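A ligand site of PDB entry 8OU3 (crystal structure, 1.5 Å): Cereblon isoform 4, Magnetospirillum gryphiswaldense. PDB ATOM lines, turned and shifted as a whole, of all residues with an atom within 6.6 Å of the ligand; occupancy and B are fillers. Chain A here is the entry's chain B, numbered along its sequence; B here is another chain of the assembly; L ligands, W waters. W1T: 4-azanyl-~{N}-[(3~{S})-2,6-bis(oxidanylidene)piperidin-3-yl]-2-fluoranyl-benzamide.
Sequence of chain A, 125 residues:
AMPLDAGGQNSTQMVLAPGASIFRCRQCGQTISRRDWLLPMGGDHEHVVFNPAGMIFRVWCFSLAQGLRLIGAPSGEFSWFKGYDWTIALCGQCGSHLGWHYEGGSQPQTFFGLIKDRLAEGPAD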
ATOM      1  N   PHE A  50      28.614  19.739 -13.037  1.00  0.00           N
ATOM      2  CA  PHE A  50      27.253  19.466 -13.488  1.00  0.00           C
ATOM      3  C   PHE A  50      26.670  18.295 -12.664  1.00  0.00           C
ATOM      4  O   PHE A  50      27.428  17.433 -12.184  1.00  0.00           O
ATOM      5  CB  PHE A  50      27.175  19.193 -14.977  1.00  0.00           C
ATOM      6  CG  PHE A  50      27.919  17.947 -15.435  1.00  0.00           C
ATOM      7  CD1 PHE A  50      27.302  16.703 -15.415  1.00  0.00           C
ATOM      8  CD2 PHE A  50      29.233  18.008 -15.870  1.00  0.00           C
ATOM      9  CE1 PHE A  50      27.970  15.576 -15.838  1.00  0.00           C
ATOM     10  CE2 PHE A  50      29.916  16.860 -16.267  1.00  0.00           C
ATOM     11  CZ  PHE A  50      29.298  15.636 -16.236  1.00  0.00           C
ATOM     12  N   ASN A  51      25.373  18.385 -12.414  1.00  0.00           N
ATOM     13  CA  ASN A  51      24.698  17.314 -11.665  1.00  0.00           C
ATOM     14  C   ASN A  51      24.152  16.260 -12.640  1.00  0.00           C
ATOM     15  O   ASN A  51      24.289  16.264 -13.875  1.00  0.00           O
ATOM     16  CB  ASN A  51      23.624  17.951 -10.781  1.00  0.00           C
ATOM     17  CG  ASN A  51      22.431  18.510 -11.499  1.00  0.00           C
ATOM     18  OD1 ASN A  51      22.166  18.225 -12.670  1.00  0.00           O
ATOM     19  ND2 ASN A  51      21.617  19.234 -10.744  1.00  0.00           N
ATOM     20  N   PRO A  52      23.534  15.157 -12.108  1.00  0.00           N
ATOM     21  CA  PRO A  52      23.037  14.110 -12.972  1.00  0.00           C
ATOM     22  C   PRO A  52      21.892  14.489 -13.931  1.00  0.00           C
ATOM     23  O   PRO A  52      21.658  13.775 -14.864  1.00  0.00           O
ATOM     24  CB  PRO A  52      22.548  13.008 -12.009  1.00  0.00           C
ATOM     25  CG  PRO A  52      23.312  13.281 -10.750  1.00  0.00           C
ATOM     26  CD  PRO A  52      23.526  14.791 -10.679  1.00  0.00           C
ATOM     27  N   ALA A  53      21.174  15.574 -13.605  1.00  0.00           N
ATOM     28  CA  ALA A  53      20.166  16.090 -14.505  1.00  0.00           C
ATOM     29  C   ALA A  53      20.766  17.037 -15.548  1.00  0.00           C
ATOM     30  O   ALA A  53      20.031  17.494 -16.424  1.00  0.00           O
ATOM     31  CB  ALA A  53      19.091  16.823 -13.697  1.00  0.00           C
ATOM     32  N   MET A  55      22.343  19.887 -15.097  1.00  0.00           N
ATOM     33  CA  MET A  55      22.418  21.303 -14.761  1.00  0.00           C
ATOM     34  C   MET A  55      23.863  21.654 -14.442  1.00  0.00           C
ATOM     35  O   MET A  55      24.534  20.955 -13.694  1.00  0.00           O
ATOM     36  CB  MET A  55      21.487  21.641 -13.587  1.00  0.00           C
ATOM     37  CG  MET A  55      20.057  21.374 -13.871  1.00  0.00           C
ATOM     38  SD  MET A  55      19.365  22.625 -15.014  1.00  0.00           S
ATOM     39  CE  MET A  55      19.348  21.629 -16.489  1.00  0.00           C
ATOM     40  N   PHE A  57      26.697  24.333 -12.802  1.00  0.00           N
ATOM     41  CA  PHE A  57      26.842  25.320 -11.761  1.00  0.00           C
ATOM     42  C   PHE A  57      28.304  25.751 -11.649  1.00  0.00           C
ATOM     43  O   PHE A  57      29.202  24.927 -11.818  1.00  0.00           O
ATOM     44  CB  PHE A  57      26.450  24.812 -10.358  1.00  0.00           C
ATOM     45  CG  PHE A  57      25.033  24.260 -10.290  1.00  0.00           C
ATOM     46  CD1 PHE A  57      23.984  25.105  -9.937  1.00  0.00           C
ATOM     47  CD2 PHE A  57      24.737  22.922 -10.530  1.00  0.00           C
ATOM     48  CE1 PHE A  57      22.682  24.644  -9.890  1.00  0.00           C
ATOM     49  CE2 PHE A  57      23.434  22.473 -10.494  1.00  0.00           C
ATOM     50  CZ  PHE A  57      22.409  23.315 -10.145  1.00  0.00           C
ATOM     51  N   GLU A  77      25.738  10.469  -2.805  1.00  0.00           N
ATOM     52  CA  GLU A  77      25.526  10.166  -4.227  1.00  0.00           C
ATOM     53  C   GLU A  77      26.008  11.343  -5.081  1.00  0.00           C
ATOM     54  O   GLU A  77      25.587  12.469  -4.858  1.00  0.00           O
ATOM     55  CB  GLU A  77      24.053   9.910  -4.531  1.00  0.00           C
ATOM     56  N   PHE A  78      26.874  11.053  -6.081  1.00  0.00           N
ATOM     57  CA  PHE A  78      27.306  12.026  -7.073  1.00  0.00           C
ATOM     58  C   PHE A  78      28.003  13.223  -6.445  1.00  0.00           C
ATOM     59  O   PHE A  78      28.085  14.312  -7.039  1.00  0.00           O
ATOM     60  CB  PHE A  78      26.129  12.534  -7.908  1.00  0.00           C
ATOM     61  CG  PHE A  78      25.205  11.477  -8.449  1.00  0.00           C
ATOM     62  CD1 PHE A  78      25.640  10.597  -9.401  1.00  0.00           C
ATOM     63  CD2 PHE A  78      23.892  11.391  -7.989  1.00  0.00           C
ATOM     64  CE1 PHE A  78      24.786   9.628  -9.897  1.00  0.00           C
ATOM     65  CE2 PHE A  78      23.039  10.422  -8.485  1.00  0.00           C
ATOM     66  CZ  PHE A  78      23.501   9.549  -9.431  1.00  0.00           C
ATOM     67  N   SER A  79      28.607  13.056  -5.253  1.00  0.00           N
ATOM     68  CA  SER A  79      29.296  14.185  -4.678  1.00  0.00           C
ATOM     69  C   SER A  79      30.392  14.693  -5.613  1.00  0.00           C
ATOM     70  O   SER A  79      31.234  13.898  -6.070  1.00  0.00           O
ATOM     71  CB  SER A  79      29.921  13.804  -3.359  1.00  0.00           C
ATOM     72  OG  SER A  79      30.518  14.950  -2.795  1.00  0.00           O
ATOM     73  N   TRP A  80      30.467  16.026  -5.755  1.00  0.00           N
ATOM     74  CA  TRP A  80      31.497  16.634  -6.578  1.00  0.00           C
ATOM     75  C   TRP A  80      32.872  16.597  -5.882  1.00  0.00           C
ATOM     76  O   TRP A  80      33.892  16.887  -6.517  1.00  0.00           O
ATOM     77  CB  TRP A  80      31.123  18.061  -6.965  1.00  0.00           C
ATOM     78  CG  TRP A  80      29.936  18.168  -7.885  1.00  0.00           C
ATOM     79  CD1 TRP A  80      29.707  17.408  -8.988  1.00  0.00           C
ATOM     80  CD2 TRP A  80      28.821  19.061  -7.767  1.00  0.00           C
ATOM     81  NE1 TRP A  80      28.542  17.807  -9.573  1.00  0.00           N
ATOM     82  CE2 TRP A  80      27.979  18.816  -8.879  1.00  0.00           C
ATOM     83  CE3 TRP A  80      28.480  20.097  -6.884  1.00  0.00           C
ATOM     84  CZ2 TRP A  80      26.785  19.516  -9.084  1.00  0.00           C
ATOM     85  CZ3 TRP A  80      27.318  20.796  -7.099  1.00  0.00           C
ATOM     86  CH2 TRP A  80      26.487  20.533  -8.205  1.00  0.00           C
ATOM     87  N   PHE A  81      32.901  16.304  -4.578  1.00  0.00           N
ATOM     88  CA  PHE A  81      34.111  16.330  -3.787  1.00  0.00           C
ATOM     89  C   PHE A  81      34.285  14.979  -3.124  1.00  0.00           C
ATOM     90  O   PHE A  81      33.541  14.621  -2.202  1.00  0.00           O
ATOM     91  CB  PHE A  81      34.074  17.514  -2.800  1.00  0.00           C
ATOM     92  CG  PHE A  81      33.934  18.857  -3.474  1.00  0.00           C
ATOM     93  CD1 PHE A  81      35.029  19.505  -4.028  1.00  0.00           C
ATOM     94  CD2 PHE A  81      32.697  19.470  -3.551  1.00  0.00           C
ATOM     95  CE1 PHE A  81      34.845  20.707  -4.702  1.00  0.00           C
ATOM     96  CE2 PHE A  81      32.527  20.690  -4.174  1.00  0.00           C
ATOM     97  CZ  PHE A  81      33.603  21.295  -4.763  1.00  0.00           C
ATOM     98  N   TRP A  86      26.860  15.542   0.879  1.00  0.00           N
ATOM     99  CA  TRP A  86      26.306  16.871   0.712  1.00  0.00           C
ATOM    100  C   TRP A  86      24.884  16.993   1.249  1.00  0.00           C
ATOM    101  O   TRP A  86      24.161  15.995   1.317  1.00  0.00           O
ATOM    102  CB  TRP A  86      26.342  17.284  -0.762  1.00  0.00           C
ATOM    103  CG  TRP A  86      25.673  16.310  -1.682  1.00  0.00           C
ATOM    104  CD1 TRP A  86      26.261  15.249  -2.332  1.00  0.00           C
ATOM    105  CD2 TRP A  86      24.283  16.242  -2.014  1.00  0.00           C
ATOM    106  NE1 TRP A  86      25.338  14.545  -3.033  1.00  0.00           N
ATOM    107  CE2 TRP A  86      24.116  15.136  -2.879  1.00  0.00           C
ATOM    108  CE3 TRP A  86      23.163  17.005  -1.682  1.00  0.00           C
ATOM    109  CZ2 TRP A  86      22.876  14.800  -3.432  1.00  0.00           C
ATOM    110  CZ3 TRP A  86      21.947  16.685  -2.227  1.00  0.00           C
ATOM    111  CH2 TRP A  86      21.797  15.568  -3.055  1.00  0.00           C
ATOM    112  N   THR A  87      24.536  18.256   1.549  1.00  0.00           N
ATOM    113  CA  THR A  87      23.169  18.669   1.892  1.00  0.00           C
ATOM    114  C   THR A  87      22.906  19.975   1.146  1.00  0.00           C
ATOM    115  O   THR A  87      23.805  20.802   1.028  1.00  0.00           O
ATOM    116  CB  THR A  87      22.977  18.868   3.408  1.00  0.00           C
ATOM    117  OG1 THR A  87      23.815  19.908   3.888  1.00  0.00           O
ATOM    118  CG2 THR A  87      23.365  17.657   4.186  1.00  0.00           C
ATOM    119  N   ILE A  88      21.688  20.146   0.629  1.00  0.00           N
ATOM    120  CA  ILE A  88      21.329  21.392  -0.049  1.00  0.00           C
ATOM    121  C   ILE A  88      21.295  22.555   0.948  1.00  0.00           C
ATOM    122  O   ILE A  88      20.776  22.415   2.048  1.00  0.00           O
ATOM    123  CB  ILE A  88      19.953  21.226  -0.735  1.00  0.00           C
ATOM    124  CG1 ILE A  88      20.029  20.213  -1.863  1.00  0.00           C
ATOM    125  CG2 ILE A  88      19.375  22.545  -1.223  1.00  0.00           C
ATOM    126  N   HIS A  97      18.182  29.166  -3.350  1.00  0.00           N
ATOM    127  CA  HIS A  97      19.127  28.049  -3.309  1.00  0.00           C
ATOM    128  C   HIS A  97      20.527  28.541  -3.568  1.00  0.00           C
ATOM    129  O   HIS A  97      20.825  28.912  -4.686  1.00  0.00           O
ATOM    130  CB  HIS A  97      18.732  26.934  -4.287  1.00  0.00           C
ATOM    131  CG  HIS A  97      19.745  25.830  -4.400  1.00  0.00           C
ATOM    132  ND1 HIS A  97      20.003  25.108  -5.554  1.00  0.00           N
ATOM    133  CD2 HIS A  97      20.576  25.342  -3.479  1.00  0.00           C
ATOM    134  CE1 HIS A  97      20.976  24.246  -5.338  1.00  0.00           C
ATOM    135  NE2 HIS A  97      21.349  24.359  -4.075  1.00  0.00           N
ATOM    136  N   TRP A 100      25.450  24.129  -1.403  1.00  0.00           N
ATOM    137  CA  TRP A 100      25.447  22.864  -0.686  1.00  0.00           C
ATOM    138  C   TRP A 100      26.469  22.961   0.432  1.00  0.00           C
ATOM    139  O   TRP A 100      27.492  23.654   0.321  1.00  0.00           O
ATOM    140  CB  TRP A 100      25.849  21.695  -1.616  1.00  0.00           C
ATOM    141  CG  TRP A 100      24.942  21.538  -2.808  1.00  0.00           C
ATOM    142  CD1 TRP A 100      23.888  20.704  -2.864  1.00  0.00           C
ATOM    143  CD2 TRP A 100      24.991  22.239  -4.074  1.00  0.00           C
ATOM    144  NE1 TRP A 100      23.245  20.809  -4.075  1.00  0.00           N
ATOM    145  CE2 TRP A 100      23.882  21.761  -4.818  1.00  0.00           C
ATOM    146  CE3 TRP A 100      25.833  23.211  -4.618  1.00  0.00           C
ATOM    147  CZ2 TRP A 100      23.637  22.169  -6.127  1.00  0.00           C
ATOM    148  CZ3 TRP A 100      25.528  23.670  -5.890  1.00  0.00           C
ATOM    149  CH2 TRP A 100      24.475  23.143  -6.620  1.00  0.00           C
ATOM    150  N   TYR A 102      29.049  20.392   2.666  1.00  0.00           N
ATOM    151  CA  TYR A 102      29.784  19.152   2.552  1.00  0.00           C
ATOM    152  C   TYR A 102      30.325  18.790   3.927  1.00  0.00           C
ATOM    153  O   TYR A 102      30.793  19.651   4.637  1.00  0.00           O
ATOM    154  CB  TYR A 102      30.932  19.244   1.539  1.00  0.00           C
ATOM    155  CG  TYR A 102      30.422  19.429   0.140  1.00  0.00           C
ATOM    156  CD1 TYR A 102      30.104  18.325  -0.625  1.00  0.00           C
ATOM    157  CD2 TYR A 102      30.217  20.691  -0.415  1.00  0.00           C
ATOM    158  CE1 TYR A 102      29.550  18.475  -1.886  1.00  0.00           C
ATOM    159  CE2 TYR A 102      29.620  20.846  -1.659  1.00  0.00           C
ATOM    160  CZ  TYR A 102      29.315  19.731  -2.395  1.00  0.00           C
ATOM    161  OH  TYR A 102      28.745  19.894  -3.634  1.00  0.00           O
ATOM    162  N   GLY B  19      31.049  11.906  -8.439  1.00  0.00           N
ATOM    163  CA  GLY B  19      30.552  13.125  -9.073  1.00  0.00           C
ATOM    164  C   GLY B  19      31.637  13.923  -9.796  1.00  0.00           C
ATOM    165  O   GLY B  19      31.389  14.994 -10.361  1.00  0.00           O
ATOM    166  N   PRO B 123      29.386  13.675 -12.890  1.00  0.00           N
ATOM    167  CA  PRO B 123      29.279  12.212 -12.853  1.00  0.00           C
ATOM    168  C   PRO B 123      29.272  11.585 -14.243  1.00  0.00           C
ATOM    169  O   PRO B 123      28.886  12.215 -15.215  1.00  0.00           O
ATOM    170  CB  PRO B 123      27.963  11.959 -12.143  1.00  0.00           C
ATOM    171  CG  PRO B 123      27.137  13.211 -12.342  1.00  0.00           C
ATOM    172  CD  PRO B 123      28.151  14.329 -12.417  1.00  0.00           C
HETATM  173  C1  W1T L   1      19.879  14.547  -8.567  1.00  0.00           C
HETATM  174  C2  W1T L   1      18.812  15.209  -9.169  1.00  0.00           C
HETATM  175  C3  W1T L   1      18.797  16.599  -9.241  1.00  0.00           C
HETATM  176  C4  W1T L   1      19.841  17.323  -8.706  1.00  0.00           C
HETATM  177  C9  W1T L   1      24.423  17.731  -5.215  1.00  0.00           C
HETATM  178  C8  W1T L   1      24.312  17.567  -6.723  1.00  0.00           C
HETATM  179  O2  W1T L   1      25.426  16.250  -8.364  1.00  0.00           O
HETATM  180  O1  W1T L   1      22.089  18.782  -7.863  1.00  0.00           O
HETATM  181  N1  W1T L   1      23.089  16.913  -7.105  1.00  0.00           N
HETATM  182  C12 W1T L   1      25.503  16.821  -7.296  1.00  0.00           C
HETATM  183  O3  W1T L   1      27.999  17.490  -4.864  1.00  0.00           O
HETATM  184  N2  W1T L   1      26.663  16.804  -6.530  1.00  0.00           N
HETATM  185  N3  W1T L   1      17.769  14.480  -9.669  1.00  0.00           N
HETATM  186  C6  W1T L   1      20.911  15.314  -8.061  1.00  0.00           C
HETATM  187  F1  W1T L   1      21.914  14.644  -7.464  1.00  0.00           F
HETATM  188  C5  W1T L   1      20.918  16.693  -8.088  1.00  0.00           C
HETATM  189  C7  W1T L   1      22.053  17.563  -7.632  1.00  0.00           C
HETATM  190  C11 W1T L   1      26.918  17.524  -5.394  1.00  0.00           C
HETATM  191  C10 W1T L   1      25.790  18.303  -4.841  1.00  0.00           C
HETATM  192  O   HOH W   1      20.900  19.588  -5.199  1.00  0.00           O
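OD1 of Asn 51 sits at hydrogen-bond distance from N of Ala 53, at 3.0 Å. OD1 of Asn 51 sits at hydrogen-bond distance from N of Met 55 (2.9 Å). NE1 of Trp 80 sits at hydrogen-bond distance from O of Phe 50 (2.9 Å). The indole nitrogen (NE1) of Trp 86 lies within hydrogen-bond range of the backbone carbonyl oxygen (O) of Glu 77, at 2.8 Å. O of Phe 81 sits at hydrogen-bond distance from OG of Ser 79 (3.1 Å). The backbone carbonyl oxygen of Ser 79 sits at hydrogen-bond distance from the backbone NH of Gly 19 of chain B.
Water W1 bridges NE1 of Trp 100 (2.9 Å) and O1 of the ligand (3.0 Å).
Residues that only touch the ligand: Pro 52, Trp 100, Trp 86 and Ser 79. Hydrophobic or aromatic side chains that line the ligand: Pro 52, Phe 78, Trp 80, Trp 86, Trp 100 and Tyr 102. Eight residues have an atom within 4 Å of the ligand: Asn 51, Pro 52, Phe 78, Ser 79, Trp 80, Trp 86, Trp 100 and Tyr 102. Along chain A the residues within 4 Å of the ligand span positions 51 to 102.
OH of Tyr 102 is in hydrogen-bond range of O3 of the ligand. The backbone carbonyl oxygen of Phe 78 sits at hydrogen-bond distance from a nitrogen (N2) of the ligand (2.9 Å). O1 of the ligand lies within hydrogen-bond range of ND2 of Asn 51, at 3.0 Å. N of Trp 80 lies within hydrogen-bond range of O3 of the ligand (3.0 Å).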
